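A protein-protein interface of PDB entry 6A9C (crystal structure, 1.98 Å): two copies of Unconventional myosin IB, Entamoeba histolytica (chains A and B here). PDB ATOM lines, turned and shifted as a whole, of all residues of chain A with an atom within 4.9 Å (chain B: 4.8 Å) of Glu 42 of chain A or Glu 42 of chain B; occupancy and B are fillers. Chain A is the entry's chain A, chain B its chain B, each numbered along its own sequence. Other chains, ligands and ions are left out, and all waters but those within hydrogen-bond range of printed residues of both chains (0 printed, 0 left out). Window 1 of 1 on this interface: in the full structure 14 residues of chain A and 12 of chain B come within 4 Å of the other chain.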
ATOM      1  N   LEU A   4     -29.423 -29.485 -10.237  1.00  0.00           N
ATOM      2  CA  LEU A   4     -29.931 -28.152 -10.536  1.00  0.00           C
ATOM      3  C   LEU A   4     -31.408 -28.102 -10.221  1.00  0.00           C
ATOM      4  O   LEU A   4     -32.112 -29.058 -10.546  1.00  0.00           O
ATOM      5  CB  LEU A   4     -29.732 -27.850 -12.039  1.00  0.00           C
ATOM      6  CG  LEU A   4     -28.246 -27.588 -12.347  1.00  0.00           C
ATOM      7  CD1 LEU A   4     -28.004 -27.657 -13.837  1.00  0.00           C
ATOM      8  CD2 LEU A   4     -27.695 -26.287 -11.766  1.00  0.00           C
ATOM      9  N   LEU A  21     -36.313 -16.251 -22.118  1.00  0.00           N
ATOM     10  CA  LEU A  21     -36.668 -17.545 -22.670  1.00  0.00           C
ATOM     11  C   LEU A  21     -38.185 -17.705 -22.736  1.00  0.00           C
ATOM     12  O   LEU A  21     -38.859 -17.537 -21.703  1.00  0.00           O
ATOM     13  CB  LEU A  21     -36.085 -18.594 -21.762  1.00  0.00           C
ATOM     14  CG  LEU A  21     -36.368 -20.034 -21.999  1.00  0.00           C
ATOM     15  CD1 LEU A  21     -35.672 -20.465 -23.254  1.00  0.00           C
ATOM     16  CD2 LEU A  21     -35.895 -20.837 -20.818  1.00  0.00           C
ATOM     17  N   ILE A  28     -40.667 -28.165 -18.550  1.00  0.00           N
ATOM     18  CA  ILE A  28     -39.810 -28.384 -17.394  1.00  0.00           C
ATOM     19  C   ILE A  28     -38.491 -27.676 -17.721  1.00  0.00           C
ATOM     20  O   ILE A  28     -37.796 -28.124 -18.614  1.00  0.00           O
ATOM     21  CB  ILE A  28     -39.430 -29.892 -17.130  1.00  0.00           C
ATOM     22  CG1 ILE A  28     -40.618 -30.706 -16.582  1.00  0.00           C
ATOM     23  CG2 ILE A  28     -38.373 -29.950 -16.003  1.00  0.00           C
ATOM     24  CD1 ILE A  28     -41.824 -30.786 -17.479  1.00  0.00           C
ATOM     25  N   ILE A  29     -38.110 -26.701 -16.916  1.00  0.00           N
ATOM     26  CA  ILE A  29     -36.982 -25.849 -17.190  1.00  0.00           C
ATOM     27  C   ILE A  29     -35.999 -26.044 -16.092  1.00  0.00           C
ATOM     28  O   ILE A  29     -36.344 -26.059 -14.923  1.00  0.00           O
ATOM     29  CB  ILE A  29     -37.465 -24.388 -17.245  1.00  0.00           C
ATOM     30  CG1 ILE A  29     -38.538 -24.245 -18.318  1.00  0.00           C
ATOM     31  CG2 ILE A  29     -36.341 -23.407 -17.527  1.00  0.00           C
ATOM     32  CD1 ILE A  29     -39.491 -23.077 -18.126  1.00  0.00           C
ATOM     33  N   THR A  30     -34.732 -26.152 -16.462  1.00  0.00           N
ATOM     34  CA  THR A  30     -33.656 -26.216 -15.518  1.00  0.00           C
ATOM     35  C   THR A  30     -33.104 -24.830 -15.232  1.00  0.00           C
ATOM     36  O   THR A  30     -32.850 -24.025 -16.184  1.00  0.00           O
ATOM     37  CB  THR A  30     -32.519 -27.106 -16.094  1.00  0.00           C
ATOM     38  OG1 THR A  30     -33.107 -28.345 -16.453  1.00  0.00           O
ATOM     39  CG2 THR A  30     -31.463 -27.332 -15.099  1.00  0.00           C
ATOM     40  N   LEU A  32     -30.280 -22.290 -13.833  1.00  0.00           N
ATOM     41  CA  LEU A  32     -28.806 -22.185 -13.787  1.00  0.00           C
ATOM     42  C   LEU A  32     -28.328 -21.085 -12.917  1.00  0.00           C
ATOM     43  O   LEU A  32     -27.237 -21.151 -12.441  1.00  0.00           O
ATOM     44  CB  LEU A  32     -28.267 -21.931 -15.199  1.00  0.00           C
ATOM     45  CG  LEU A  32     -28.752 -22.902 -16.287  1.00  0.00           C
ATOM     46  CD1 LEU A  32     -28.317 -22.528 -17.712  1.00  0.00           C
ATOM     47  CD2 LEU A  32     -28.257 -24.294 -15.973  1.00  0.00           C
ATOM     48  N   LYS A  40     -32.430 -17.656 -14.504  1.00  0.00           N
ATOM     49  CA  LYS A  40     -31.911 -18.031 -15.799  1.00  0.00           C
ATOM     50  C   LYS A  40     -32.141 -19.499 -16.067  1.00  0.00           C
ATOM     51  O   LYS A  40     -31.644 -20.373 -15.364  1.00  0.00           O
ATOM     52  CB  LYS A  40     -30.445 -17.595 -15.916  1.00  0.00           C
ATOM     53  CG  LYS A  40     -29.855 -17.691 -17.332  1.00  0.00           C
ATOM     54  CD  LYS A  40     -28.410 -17.130 -17.398  1.00  0.00           C
ATOM     55  CE  LYS A  40     -28.144 -16.586 -18.785  1.00  0.00           C
ATOM     56  NZ  LYS A  40     -26.844 -15.891 -18.863  1.00  0.00           N
ATOM     57  N   GLY A  41     -32.948 -19.786 -17.071  1.00  0.00           N
ATOM     58  CA  GLY A  41     -33.374 -21.160 -17.317  1.00  0.00           C
ATOM     59  C   GLY A  41     -32.827 -21.727 -18.602  1.00  0.00           C
ATOM     60  O   GLY A  41     -32.372 -20.977 -19.505  1.00  0.00           O
ATOM     61  N   GLU A  42     -32.940 -23.045 -18.712  1.00  0.00           N
ATOM     62  CA  GLU A  42     -32.497 -23.811 -19.870  1.00  0.00           C
ATOM     63  C   GLU A  42     -33.566 -24.831 -20.284  1.00  0.00           C
ATOM     64  O   GLU A  42     -34.095 -25.555 -19.478  1.00  0.00           O
ATOM     65  CB  GLU A  42     -31.144 -24.505 -19.576  1.00  0.00           C
ATOM     66  CG  GLU A  42     -30.664 -25.391 -20.749  1.00  0.00           C
ATOM     67  CD  GLU A  42     -31.291 -26.801 -20.808  1.00  0.00           C
ATOM     68  OE1 GLU A  42     -31.265 -27.485 -19.771  1.00  0.00           O
ATOM     69  OE2 GLU A  42     -31.804 -27.234 -21.907  1.00  0.00           O
ATOM     70  N   LEU A  43     -33.965 -24.817 -21.522  1.00  0.00           N
ATOM     71  CA  LEU A  43     -35.052 -25.664 -21.979  1.00  0.00           C
ATOM     72  C   LEU A  43     -34.725 -26.047 -23.410  1.00  0.00           C
ATOM     73  O   LEU A  43     -34.699 -25.183 -24.324  1.00  0.00           O
ATOM     74  CB  LEU A  43     -36.398 -24.883 -21.944  1.00  0.00           C
ATOM     75  CG  LEU A  43     -37.611 -25.523 -22.613  1.00  0.00           C
ATOM     76  CD1 LEU A  43     -38.080 -26.723 -21.778  1.00  0.00           C
ATOM     77  CD2 LEU A  43     -38.761 -24.528 -22.838  1.00  0.00           C
ATOM     78  N   ASN A  44     -34.517 -27.345 -23.637  1.00  0.00           N
ATOM     79  CA  ASN A  44     -34.168 -27.871 -24.980  1.00  0.00           C
ATOM     80  C   ASN A  44     -33.005 -27.138 -25.612  1.00  0.00           C
ATOM     81  O   ASN A  44     -33.029 -26.823 -26.803  1.00  0.00           O
ATOM     82  CB  ASN A  44     -35.387 -27.848 -25.924  1.00  0.00           C
ATOM     83  CG  ASN A  44     -36.577 -28.606 -25.340  1.00  0.00           C
ATOM     84  OD1 ASN A  44     -36.412 -29.515 -24.516  1.00  0.00           O
ATOM     85  ND2 ASN A  44     -37.781 -28.203 -25.715  1.00  0.00           N
ATOM     86  N   GLY A  45     -32.025 -26.821 -24.782  1.00  0.00           N
ATOM     87  CA  GLY A  45     -30.816 -26.246 -25.225  1.00  0.00           C
ATOM     88  C   GLY A  45     -30.809 -24.743 -25.353  1.00  0.00           C
ATOM     89  O   GLY A  45     -29.803 -24.195 -25.694  1.00  0.00           O
ATOM     90  N   GLN A  46     -31.922 -24.103 -25.055  1.00  0.00           N
ATOM     91  CA  GLN A  46     -32.106 -22.652 -25.161  1.00  0.00           C
ATOM     92  C   GLN A  46     -32.024 -22.140 -23.756  1.00  0.00           C
ATOM     93  O   GLN A  46     -32.644 -22.691 -22.843  1.00  0.00           O
ATOM     94  CB  GLN A  46     -33.497 -22.292 -25.720  1.00  0.00           C
ATOM     95  CG  GLN A  46     -33.868 -22.698 -27.129  1.00  0.00           C
ATOM     96  CD  GLN A  46     -33.134 -21.885 -28.181  1.00  0.00           C
ATOM     97  OE1 GLN A  46     -32.584 -22.457 -29.086  1.00  0.00           O
ATOM     98  NE2 GLN A  46     -33.128 -20.570 -28.075  1.00  0.00           N
ATOM     99  N   GLU A  47     -31.290 -21.059 -23.586  1.00  0.00           N
ATOM    100  CA  GLU A  47     -31.088 -20.464 -22.294  1.00  0.00           C
ATOM    101  C   GLU A  47     -31.534 -19.021 -22.249  1.00  0.00           C
ATOM    102  O   GLU A  47     -31.219 -18.242 -23.167  1.00  0.00           O
ATOM    103  CB  GLU A  47     -29.595 -20.563 -21.999  1.00  0.00           C
ATOM    104  CG  GLU A  47     -29.055 -19.773 -20.855  1.00  0.00           C
ATOM    105  CD  GLU A  47     -27.541 -19.672 -20.950  1.00  0.00           C
ATOM    106  OE1 GLU A  47     -27.014 -19.168 -21.962  1.00  0.00           O
ATOM    107  OE2 GLU A  47     -26.888 -20.107 -19.998  1.00  0.00           O
ATOM    108  N   LEU B   4     -27.398 -23.056 -26.379  1.00  0.00           N
ATOM    109  CA  LEU B   4     -26.149 -23.560 -25.844  1.00  0.00           C
ATOM    110  C   LEU B   4     -25.719 -24.744 -26.708  1.00  0.00           C
ATOM    111  O   LEU B   4     -26.583 -25.457 -27.278  1.00  0.00           O
ATOM    112  CB  LEU B   4     -26.330 -23.988 -24.379  1.00  0.00           C
ATOM    113  CG  LEU B   4     -26.570 -22.888 -23.343  1.00  0.00           C
ATOM    114  CD1 LEU B   4     -27.207 -23.455 -22.090  1.00  0.00           C
ATOM    115  CD2 LEU B   4     -25.291 -22.094 -22.977  1.00  0.00           C
ATOM    116  N   LEU B  21     -20.091 -36.044 -14.347  1.00  0.00           N
ATOM    117  CA  LEU B  21     -21.451 -36.335 -14.697  1.00  0.00           C
ATOM    118  C   LEU B  21     -21.484 -37.643 -15.402  1.00  0.00           C
ATOM    119  O   LEU B  21     -20.869 -37.780 -16.489  1.00  0.00           O
ATOM    120  CB  LEU B  21     -21.962 -35.228 -15.627  1.00  0.00           C
ATOM    121  CG  LEU B  21     -23.344 -35.382 -16.294  1.00  0.00           C
ATOM    122  CD1 LEU B  21     -24.404 -35.439 -15.207  1.00  0.00           C
ATOM    123  CD2 LEU B  21     -23.719 -34.338 -17.325  1.00  0.00           C
ATOM    124  N   ILE B  28     -28.372 -36.692 -24.657  1.00  0.00           N
ATOM    125  CA  ILE B  28     -28.212 -35.353 -25.169  1.00  0.00           C
ATOM    126  C   ILE B  28     -27.877 -34.425 -24.003  1.00  0.00           C
ATOM    127  O   ILE B  28     -28.695 -34.160 -23.128  1.00  0.00           O
ATOM    128  CB  ILE B  28     -29.447 -34.817 -25.885  1.00  0.00           C
ATOM    129  CG1 ILE B  28     -29.892 -35.770 -27.027  1.00  0.00           C
ATOM    130  CG2 ILE B  28     -29.142 -33.406 -26.436  1.00  0.00           C
ATOM    131  CD1 ILE B  28     -28.893 -35.904 -28.146  1.00  0.00           C
ATOM    132  N   ILE B  29     -26.636 -33.960 -23.990  1.00  0.00           N
ATOM    133  CA  ILE B  29     -26.107 -33.208 -22.865  1.00  0.00           C
ATOM    134  C   ILE B  29     -25.888 -31.761 -23.337  1.00  0.00           C
ATOM    135  O   ILE B  29     -25.310 -31.528 -24.368  1.00  0.00           O
ATOM    136  CB  ILE B  29     -24.843 -33.827 -22.383  1.00  0.00           C
ATOM    137  CG1 ILE B  29     -25.143 -35.302 -22.091  1.00  0.00           C
ATOM    138  CG2 ILE B  29     -24.265 -33.045 -21.200  1.00  0.00           C
ATOM    139  CD1 ILE B  29     -23.917 -36.126 -21.946  1.00  0.00           C
ATOM    140  N   THR B  30     -26.317 -30.800 -22.526  1.00  0.00           N
ATOM    141  CA  THR B  30     -26.155 -29.399 -22.847  1.00  0.00           C
ATOM    142  C   THR B  30     -24.874 -28.923 -22.192  1.00  0.00           C
ATOM    143  O   THR B  30     -24.629 -29.242 -21.026  1.00  0.00           O
ATOM    144  CB  THR B  30     -27.352 -28.587 -22.285  1.00  0.00           C
ATOM    145  OG1 THR B  30     -28.557 -29.117 -22.835  1.00  0.00           O
ATOM    146  CG2 THR B  30     -27.232 -27.172 -22.695  1.00  0.00           C
ATOM    147  N   LEU B  32     -22.322 -26.222 -20.732  1.00  0.00           N
ATOM    148  CA  LEU B  32     -22.273 -24.950 -20.031  1.00  0.00           C
ATOM    149  C   LEU B  32     -20.921 -24.302 -20.163  1.00  0.00           C
ATOM    150  O   LEU B  32     -20.825 -23.075 -20.079  1.00  0.00           O
ATOM    151  CB  LEU B  32     -22.551 -25.186 -18.566  1.00  0.00           C
ATOM    152  CG  LEU B  32     -23.864 -25.956 -18.349  1.00  0.00           C
ATOM    153  CD1 LEU B  32     -24.180 -26.164 -16.861  1.00  0.00           C
ATOM    154  CD2 LEU B  32     -25.011 -25.226 -19.010  1.00  0.00           C
ATOM    155  N   LYS B  40     -18.234 -29.036 -19.208  1.00  0.00           N
ATOM    156  CA  LYS B  40     -19.207 -29.045 -18.142  1.00  0.00           C
ATOM    157  C   LYS B  40     -20.582 -29.123 -18.758  1.00  0.00           C
ATOM    158  O   LYS B  40     -20.941 -28.294 -19.576  1.00  0.00           O
ATOM    159  CB  LYS B  40     -19.103 -27.831 -17.245  1.00  0.00           C
ATOM    160  CG  LYS B  40     -19.891 -27.958 -15.948  1.00  0.00           C
ATOM    161  CD  LYS B  40     -19.620 -26.731 -15.063  1.00  0.00           C
ATOM    162  CE  LYS B  40     -20.229 -26.995 -13.709  1.00  0.00           C
ATOM    163  NZ  LYS B  40     -20.213 -25.780 -12.860  1.00  0.00           N
ATOM    164  N   GLY B  41     -21.333 -30.162 -18.395  1.00  0.00           N
ATOM    165  CA  GLY B  41     -22.591 -30.434 -19.042  1.00  0.00           C
ATOM    166  C   GLY B  41     -23.692 -30.503 -18.039  1.00  0.00           C
ATOM    167  O   GLY B  41     -23.406 -30.623 -16.815  1.00  0.00           O
ATOM    168  N   GLU B  42     -24.918 -30.507 -18.568  1.00  0.00           N
ATOM    169  CA  GLU B  42     -26.141 -30.611 -17.800  1.00  0.00           C
ATOM    170  C   GLU B  42     -27.077 -31.615 -18.515  1.00  0.00           C
ATOM    171  O   GLU B  42     -27.262 -31.564 -19.726  1.00  0.00           O
ATOM    172  CB  GLU B  42     -26.751 -29.198 -17.700  1.00  0.00           C
ATOM    173  CG  GLU B  42     -28.122 -29.098 -17.070  1.00  0.00           C
ATOM    174  CD  GLU B  42     -29.253 -29.430 -18.020  1.00  0.00           C
ATOM    175  OE1 GLU B  42     -29.288 -28.723 -19.066  1.00  0.00           O
ATOM    176  OE2 GLU B  42     -30.073 -30.353 -17.692  1.00  0.00           O
ATOM    177  N   LEU B  43     -27.621 -32.570 -17.766  1.00  0.00           N
ATOM    178  CA  LEU B  43     -28.507 -33.583 -18.326  1.00  0.00           C
ATOM    179  C   LEU B  43     -29.526 -33.878 -17.220  1.00  0.00           C
ATOM    180  O   LEU B  43     -29.102 -34.218 -16.121  1.00  0.00           O
ATOM    181  CB  LEU B  43     -27.651 -34.805 -18.607  1.00  0.00           C
ATOM    182  CG  LEU B  43     -28.418 -36.055 -19.003  1.00  0.00           C
ATOM    183  CD1 LEU B  43     -29.122 -35.840 -20.317  1.00  0.00           C
ATOM    184  CD2 LEU B  43     -27.475 -37.236 -19.089  1.00  0.00           C
ATOM    185  N   ASN B  44     -30.809 -33.686 -17.474  1.00  0.00           N
ATOM    186  CA  ASN B  44     -31.898 -34.047 -16.509  1.00  0.00           C
ATOM    187  C   ASN B  44     -31.689 -33.564 -15.102  1.00  0.00           C
ATOM    188  O   ASN B  44     -31.817 -34.286 -14.111  1.00  0.00           O
ATOM    189  CB  ASN B  44     -32.116 -35.564 -16.551  1.00  0.00           C
ATOM    190  CG  ASN B  44     -32.472 -36.049 -17.960  1.00  0.00           C
ATOM    191  OD1 ASN B  44     -33.070 -35.320 -18.751  1.00  0.00           O
ATOM    192  ND2 ASN B  44     -32.089 -37.270 -18.288  1.00  0.00           N
ATOM    193  N   GLY B  45     -31.302 -32.301 -15.020  1.00  0.00           N
ATOM    194  CA  GLY B  45     -31.113 -31.646 -13.789  1.00  0.00           C
ATOM    195  C   GLY B  45     -29.833 -31.956 -13.047  1.00  0.00           C
ATOM    196  O   GLY B  45     -29.711 -31.499 -11.929  1.00  0.00           O
ATOM    197  N   GLN B  46     -28.905 -32.706 -13.659  1.00  0.00           N
ATOM    198  CA  GLN B  46     -27.642 -33.053 -13.033  1.00  0.00           C
ATOM    199  C   GLN B  46     -26.596 -32.328 -13.841  1.00  0.00           C
ATOM    200  O   GLN B  46     -26.705 -32.322 -15.073  1.00  0.00           O
ATOM    201  CB  GLN B  46     -27.422 -34.535 -13.091  1.00  0.00           C
ATOM    202  CG  GLN B  46     -28.485 -35.344 -12.352  1.00  0.00           C
ATOM    203  CD  GLN B  46     -28.309 -35.244 -10.862  1.00  0.00           C
ATOM    204  OE1 GLN B  46     -29.235 -34.865 -10.167  1.00  0.00           O
ATOM    205  NE2 GLN B  46     -27.090 -35.538 -10.360  1.00  0.00           N
ATOM    206  N   GLU B  47     -25.639 -31.706 -13.163  1.00  0.00           N
ATOM    207  CA  GLU B  47     -24.577 -30.963 -13.828  1.00  0.00           C
ATOM    208  C   GLU B  47     -23.197 -31.479 -13.370  1.00  0.00           C
ATOM    209  O   GLU B  47     -23.008 -31.826 -12.221  1.00  0.00           O
ATOM    210  CB  GLU B  47     -24.791 -29.509 -13.514  1.00  0.00           C
ATOM    211  CG  GLU B  47     -23.624 -28.615 -13.707  1.00  0.00           C
ATOM    212  CD  GLU B  47     -23.843 -27.316 -12.947  1.00  0.00           C
ATOM    213  OE1 GLU B  47     -24.038 -27.370 -11.698  1.00  0.00           O
ATOM    214  OE2 GLU B  47     -23.811 -26.270 -13.605  1.00  0.00           O
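Leu 4 of chain A touches Glu 42 of chain B, but with the chains exchanged Glu 42 of chain A does not touch Leu 4 of chain B (4.2 Å).
Leu 4 of chain A touches Gly 45 of chain B, and with the chains exchanged Gly 45 of chain A touches Leu 4 of chain B.
Thr 30 of chain A touches Glu 42 of chain B, and with the chains exchanged Glu 42 of chain A touches Thr 30 of chain B.
Glu 42 of chain A touches its own counterpart, Glu 42 of chain B.
Leu 4 of chain A touches Glu 42 of chain B.
Glu 47 of chain B touches Leu 4 of chain A.
OE2 of Glu 42 of chain B touches OG1 of Thr 30 of chain A (3.8 Å).
OG1 of Thr 30 of chain B touches OE2 of Glu 42 of chain A, 3.9 Å away.
Glu 47 of chain A touches Leu 4 of chain B (OE1 to CD2, 3.5 Å).
Of the 14 printed residues of chain B, 5 touch a printed residue of chain A.
Printed residues of chain A that touch a printed residue of chain B: Leu 4, Thr 30, Glu 42, Gly 45 and Glu 47.
Hydrophobic or aromatic side chains of chain A that line the printed part of chain B: Leu 4.
Of the printed residues of chain B, Leu 4 of chain A touches Glu 42 (3.5 Å), Gly 45 (2.6 Å) and Glu 47 (3.7 Å).
Glu 42 of chain A touches just these residues of chain B: Thr 30 (3.9 Å) and Glu 42 (2.4 Å).
Printed residues of chain B within 4 Å of Gly 45 of chain A: Leu 4 (2.7 Å).
Of the printed residues of chain B, Glu 47 of chain A touches Leu 4 (3.5 Å).
Ile 28 of chain B touches none of the printed residues of chain A.
Of the printed residues of chain A, Thr 30 of chain B touches Glu 42.
Glu 42 of chain B touches three residues of chain A.
Asn 44 of chain B touches none of the printed residues of chain A.
Of the printed residues of chain A, Glu 47 of chain B touches Leu 4 (3.7 Å).
The nearest printed residue of chain A that does not touch Glu 42 of chain B is Leu 32 of chain A (4.9 Å).
The nearest printed residue of chain B that does not touch Gly 45 of chain A is Thr 30 of chain B (4.4 Å).
The backbone NH (N) of Glu 42 of chain B sits at hydrogen-bond distance from the backbone carbonyl oxygen (O) of Thr 30 of chain B (2.8 Å).
The side-chain amino group (NZ) of Lys 40 of chain B is in salt-bridge range of the side-chain carboxylate (OE2) of Glu 47 of chain B, at 3.7 Å.
The backbone NH (N) of Asn 44 of chain B sits at hydrogen-bond distance from the side-chain carboxylate (OE2) of Glu 42 of chain B.
The backbone carbonyl oxygen (O) of Thr 30 of chain A lies within hydrogen-bond range of the backbone NH (N) of Glu 42 of chain A (2.7 Å).
N of Asn 44 of chain A lies within hydrogen-bond range of OE2 of Glu 42 of chain A, at 3.2 Å.
The backbone NH (N) of Gly 45 of chain A is in hydrogen-bond range of the side-chain carboxylate (OE2) of Glu 42 of chain A (2.9 Å).
The backbone NH (N) of Leu 4 of chain B sits at hydrogen-bond distance from the backbone carbonyl oxygen (O) of Gly 45 of chain A (2.7 Å).
OE1 of Glu 42 of chain A lies close to OE1 of Glu 42 of chain B, 2.4 Å away.
N of Leu 4 of chain A lies within hydrogen-bond range of O of Gly 45 of chain B.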
